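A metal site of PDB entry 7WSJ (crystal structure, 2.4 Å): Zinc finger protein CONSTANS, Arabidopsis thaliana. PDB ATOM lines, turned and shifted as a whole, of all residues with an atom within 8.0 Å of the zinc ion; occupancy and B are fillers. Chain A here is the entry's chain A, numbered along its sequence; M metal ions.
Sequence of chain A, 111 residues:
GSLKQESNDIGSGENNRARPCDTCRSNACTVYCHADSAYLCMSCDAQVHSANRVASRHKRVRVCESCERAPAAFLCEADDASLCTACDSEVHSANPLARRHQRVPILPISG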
ATOM      1  N   VAL A  63      -4.416   3.059  13.050  1.00  0.00           N
ATOM      2  CA  VAL A  63      -4.582   1.704  13.571  1.00  0.00           C
ATOM      3  C   VAL A  63      -3.289   0.928  13.387  1.00  0.00           C
ATOM      4  O   VAL A  63      -2.539   1.158  12.430  1.00  0.00           O
ATOM      5  CB  VAL A  63      -5.790   1.018  12.893  1.00  0.00           C
ATOM      6  CG1 VAL A  63      -5.849  -0.463  13.231  1.00  0.00           C
ATOM      7  CG2 VAL A  63      -7.072   1.693  13.299  1.00  0.00           C
ATOM      8  N   CYS A  64      -3.016   0.014  14.323  1.00  0.00           N
ATOM      9  CA  CYS A  64      -1.827  -0.823  14.250  1.00  0.00           C
ATOM     10  C   CYS A  64      -1.706  -1.484  12.893  1.00  0.00           C
ATOM     11  O   CYS A  64      -2.688  -1.969  12.327  1.00  0.00           O
ATOM     12  CB  CYS A  64      -1.883  -1.875  15.360  1.00  0.00           C
ATOM     13  SG  CYS A  64      -0.576  -3.129  15.286  1.00  0.00           S
ATOM     14  N   GLU A  65      -0.486  -1.497  12.359  1.00  0.00           N
ATOM     15  CA  GLU A  65      -0.260  -2.037  11.023  1.00  0.00           C
ATOM     16  C   GLU A  65      -0.105  -3.544  11.007  1.00  0.00           C
ATOM     17  O   GLU A  65      -0.167  -4.153   9.932  1.00  0.00           O
ATOM     18  CB  GLU A  65       0.969  -1.379  10.389  1.00  0.00           C
ATOM     19  CG  GLU A  65       0.842   0.127  10.217  1.00  0.00           C
ATOM     20  CD  GLU A  65       2.099   0.767   9.657  1.00  0.00           C
ATOM     21  OE1 GLU A  65       2.902   0.054   9.012  1.00  0.00           O
ATOM     22  OE2 GLU A  65       2.292   1.979   9.859  1.00  0.00           O
ATOM     23  N   SER A  66       0.100  -4.167  12.171  1.00  0.00           N
ATOM     24  CA  SER A  66       0.237  -5.625  12.234  1.00  0.00           C
ATOM     25  C   SER A  66      -1.138  -6.283  12.370  1.00  0.00           C
ATOM     26  O   SER A  66      -1.587  -6.992  11.456  1.00  0.00           O
ATOM     27  CB  SER A  66       1.161  -6.024  13.394  1.00  0.00           C
ATOM     28  OG  SER A  66       1.299  -7.428  13.462  1.00  0.00           O
ATOM     29  N   CYS A  67      -1.805  -6.061  13.501  1.00  0.00           N
ATOM     30  CA  CYS A  67      -3.079  -6.717  13.744  1.00  0.00           C
ATOM     31  C   CYS A  67      -4.235  -6.007  13.044  1.00  0.00           C
ATOM     32  O   CYS A  67      -5.253  -6.647  12.735  1.00  0.00           O
ATOM     33  CB  CYS A  67      -3.348  -6.808  15.251  1.00  0.00           C
ATOM     34  SG  CYS A  67      -3.556  -5.226  16.100  1.00  0.00           S
ATOM     35  N   GLU A  68      -4.089  -4.718  12.758  1.00  0.00           N
ATOM     36  CA  GLU A  68      -5.132  -3.900  12.131  1.00  0.00           C
ATOM     37  C   GLU A  68      -6.420  -3.873  12.944  1.00  0.00           C
ATOM     38  O   GLU A  68      -7.498  -3.630  12.394  1.00  0.00           O
ATOM     39  CB  GLU A  68      -5.417  -4.353  10.693  1.00  0.00           C
ATOM     40  CG  GLU A  68      -4.187  -4.370   9.797  1.00  0.00           C
ATOM     41  CD  GLU A  68      -4.472  -4.973   8.430  1.00  0.00           C
ATOM     42  OE1 GLU A  68      -4.551  -4.206   7.449  1.00  0.00           O
ATOM     43  OE2 GLU A  68      -4.613  -6.213   8.346  1.00  0.00           O
ATOM     44  N   ARG A  69      -6.319  -4.109  14.254  1.00  0.00           N
ATOM     45  CA  ARG A  69      -7.483  -4.137  15.126  1.00  0.00           C
ATOM     46  C   ARG A  69      -7.359  -3.264  16.356  1.00  0.00           C
ATOM     47  O   ARG A  69      -8.306  -3.187  17.145  1.00  0.00           O
ATOM     48  CB  ARG A  69      -7.787  -5.578  15.571  1.00  0.00           C
ATOM     49  CG  ARG A  69      -7.861  -6.587  14.450  1.00  0.00           C
ATOM     50  CD  ARG A  69      -8.360  -7.928  14.950  1.00  0.00           C
ATOM     51  NE  ARG A  69      -9.662  -7.796  15.599  1.00  0.00           N
ATOM     52  CZ  ARG A  69     -10.812  -7.767  14.952  1.00  0.00           C
ATOM     53  NH1 ARG A  69     -10.836  -7.854  13.626  1.00  0.00           N
ATOM     54  NH2 ARG A  69     -11.957  -7.636  15.625  1.00  0.00           N
ATOM     55  N   ALA A  70      -6.229  -2.599  16.560  1.00  0.00           N
ATOM     56  CA  ALA A  70      -5.923  -1.883  17.783  1.00  0.00           C
ATOM     57  C   ALA A  70      -5.278  -0.551  17.448  1.00  0.00           C
ATOM     58  O   ALA A  70      -4.723  -0.389  16.347  1.00  0.00           O
ATOM     59  CB  ALA A  70      -4.987  -2.716  18.680  1.00  0.00           C
ATOM     60  N   PRO A  71      -5.331   0.421  18.350  1.00  0.00           N
ATOM     61  CA  PRO A  71      -4.710   1.716  18.060  1.00  0.00           C
ATOM     62  C   PRO A  71      -3.196   1.602  18.120  1.00  0.00           C
ATOM     63  O   PRO A  71      -2.632   0.951  19.007  1.00  0.00           O
ATOM     64  CB  PRO A  71      -5.244   2.644  19.162  1.00  0.00           C
ATOM     65  CG  PRO A  71      -6.257   1.831  19.930  1.00  0.00           C
ATOM     66  CD  PRO A  71      -5.930   0.400  19.697  1.00  0.00           C
ATOM     67  N   ALA A  72      -2.528   2.250  17.170  1.00  0.00           N
ATOM     68  CA  ALA A  72      -1.068   2.254  17.157  1.00  0.00           C
ATOM     69  C   ALA A  72      -0.542   3.029  18.353  1.00  0.00           C
ATOM     70  O   ALA A  72      -1.021   4.129  18.657  1.00  0.00           O
ATOM     71  CB  ALA A  72      -0.549   2.856  15.855  1.00  0.00           C
ATOM     72  N   ALA A  73       0.462   2.473  19.028  1.00  0.00           N
ATOM     73  CA  ALA A  73       1.046   3.103  20.194  1.00  0.00           C
ATOM     74  C   ALA A  73       2.527   3.405  20.052  1.00  0.00           C
ATOM     75  O   ALA A  73       3.020   4.297  20.760  1.00  0.00           O
ATOM     76  CB  ALA A  73       0.859   2.229  21.442  1.00  0.00           C
ATOM     77  N   SER A  82       3.905   1.140  12.588  1.00  0.00           N
ATOM     78  CA  SER A  82       3.221   1.706  13.743  1.00  0.00           C
ATOM     79  C   SER A  82       2.379   0.601  14.367  1.00  0.00           C
ATOM     80  O   SER A  82       1.460   0.076  13.724  1.00  0.00           O
ATOM     81  CB  SER A  82       2.352   2.892  13.352  1.00  0.00           C
ATOM     82  OG  SER A  82       3.129   3.910  12.741  1.00  0.00           O
ATOM     83  N   LEU A  83       2.692   0.230  15.607  1.00  0.00           N
ATOM     84  CA  LEU A  83       2.117  -0.950  16.234  1.00  0.00           C
ATOM     85  C   LEU A  83       1.418  -0.592  17.542  1.00  0.00           C
ATOM     86  O   LEU A  83       1.783   0.382  18.216  1.00  0.00           O
ATOM     87  CB  LEU A  83       3.204  -1.994  16.516  1.00  0.00           C
ATOM     88  CG  LEU A  83       4.033  -2.399  15.295  1.00  0.00           C
ATOM     89  CD1 LEU A  83       5.211  -3.276  15.697  1.00  0.00           C
ATOM     90  CD2 LEU A  83       3.160  -3.112  14.280  1.00  0.00           C
ATOM     91  N   CYS A  84       0.420  -1.399  17.898  1.00  0.00           N
ATOM     92  CA  CYS A  84      -0.135  -1.326  19.241  1.00  0.00           C
ATOM     93  C   CYS A  84       0.848  -1.917  20.246  1.00  0.00           C
ATOM     94  O   CYS A  84       1.855  -2.538  19.881  1.00  0.00           O
ATOM     95  CB  CYS A  84      -1.486  -2.046  19.304  1.00  0.00           C
ATOM     96  SG  CYS A  84      -1.420  -3.819  19.005  1.00  0.00           S
ATOM     97  N   THR A  85       0.547  -1.719  21.533  1.00  0.00           N
ATOM     98  CA  THR A  85       1.470  -2.133  22.584  1.00  0.00           C
ATOM     99  C   THR A  85       1.720  -3.643  22.536  1.00  0.00           C
ATOM    100  O   THR A  85       2.866  -4.091  22.665  1.00  0.00           O
ATOM    101  CB  THR A  85       0.917  -1.732  23.959  1.00  0.00           C
ATOM    102  OG1 THR A  85       0.738  -0.319  23.991  1.00  0.00           O
ATOM    103  CG2 THR A  85       1.879  -2.146  25.061  1.00  0.00           C
ATOM    104  N   ALA A  86       0.662  -4.431  22.349  1.00  0.00           N
ATOM    105  CA  ALA A  86       0.795  -5.874  22.295  1.00  0.00           C
ATOM    106  C   ALA A  86       1.639  -6.307  21.107  1.00  0.00           C
ATOM    107  O   ALA A  86       2.550  -7.128  21.237  1.00  0.00           O
ATOM    108  CB  ALA A  86      -0.582  -6.534  22.249  1.00  0.00           C
ATOM    109  N   CYS A  87       1.335  -5.771  19.918  1.00  0.00           N
ATOM    110  CA  CYS A  87       2.121  -6.116  18.731  1.00  0.00           C
ATOM    111  C   CYS A  87       3.559  -5.615  18.865  1.00  0.00           C
ATOM    112  O   CYS A  87       4.493  -6.281  18.421  1.00  0.00           O
ATOM    113  CB  CYS A  87       1.473  -5.559  17.478  1.00  0.00           C
ATOM    114  SG  CYS A  87       0.031  -6.492  16.899  1.00  0.00           S
ATOM    115  N   ASP A  88       3.745  -4.446  19.486  1.00  0.00           N
ATOM    116  CA  ASP A  88       5.092  -3.934  19.712  1.00  0.00           C
ATOM    117  C   ASP A  88       5.900  -4.911  20.562  1.00  0.00           C
ATOM    118  O   ASP A  88       7.026  -5.294  20.190  1.00  0.00           O
ATOM    119  CB  ASP A  88       5.012  -2.570  20.380  1.00  0.00           C
ATOM    120  CG  ASP A  88       6.373  -1.962  20.635  1.00  0.00           C
ATOM    121  OD1 ASP A  88       7.120  -1.757  19.665  1.00  0.00           O
ATOM    122  OD2 ASP A  88       6.681  -1.690  21.815  1.00  0.00           O
ATOM    123  N   GLU A  90       5.279  -8.128  21.158  1.00  0.00           N
ATOM    124  CA  GLU A  90       5.435  -9.416  20.495  1.00  0.00           C
ATOM    125  C   GLU A  90       6.502  -9.363  19.417  1.00  0.00           C
ATOM    126  O   GLU A  90       7.254 -10.331  19.223  1.00  0.00           O
ATOM    127  CB  GLU A  90       4.095  -9.866  19.905  1.00  0.00           C
ATOM    128  CG  GLU A  90       4.170 -11.119  19.044  1.00  0.00           C
ATOM    129  CD  GLU A  90       2.798 -11.606  18.622  1.00  0.00           C
ATOM    130  OE1 GLU A  90       1.830 -11.404  19.392  1.00  0.00           O
ATOM    131  OE2 GLU A  90       2.678 -12.184  17.519  1.00  0.00           O
ATOM    132  N   VAL A  91       6.591  -8.254  18.692  1.00  0.00           N
ATOM    133  CA  VAL A  91       7.584  -8.121  17.632  1.00  0.00           C
ATOM    134  C   VAL A  91       8.981  -7.989  18.217  1.00  0.00           C
ATOM    135  O   VAL A  91       9.933  -8.636  17.763  1.00  0.00           O
ATOM    136  CB  VAL A  91       7.231  -6.942  16.716  1.00  0.00           C
ATOM    137  CG1 VAL A  91       8.430  -6.564  15.857  1.00  0.00           C
ATOM    138  CG2 VAL A  91       6.042  -7.292  15.837  1.00  0.00           C
HETATM  139 ZN    ZN M   1      -1.403  -4.667  16.836  1.00  0.00          ZN
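The side-chain hydroxyl (OG) of Ser 66 lies close to the side-chain sulfur (SG) of Cys 87. O of Ala 70 sits at hydrogen-bond distance from N of Cys 64, at 2.7 Å. The backbone NH (N) of Ser 66 sits close to the side-chain sulfur (SG) of Cys 64, at 3.4 Å. N of Ala 70 sits close to SG of Cys 67 (3.8 Å). SG of Cys 67 sits close to N of Arg 69, at 3.5 Å.
Of the 20 residues printed, 4 come within 4 Å of the zinc ion.
The zinc ion is bound by the side-chain sulfur (SG) of Cys 87, the side-chain sulfur (SG) of Cys 84, the side-chain sulfur (SG) of Cys 64 and the side-chain sulfur (SG) of Cys 67. The zinc ion has four donor atoms within binding distance.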
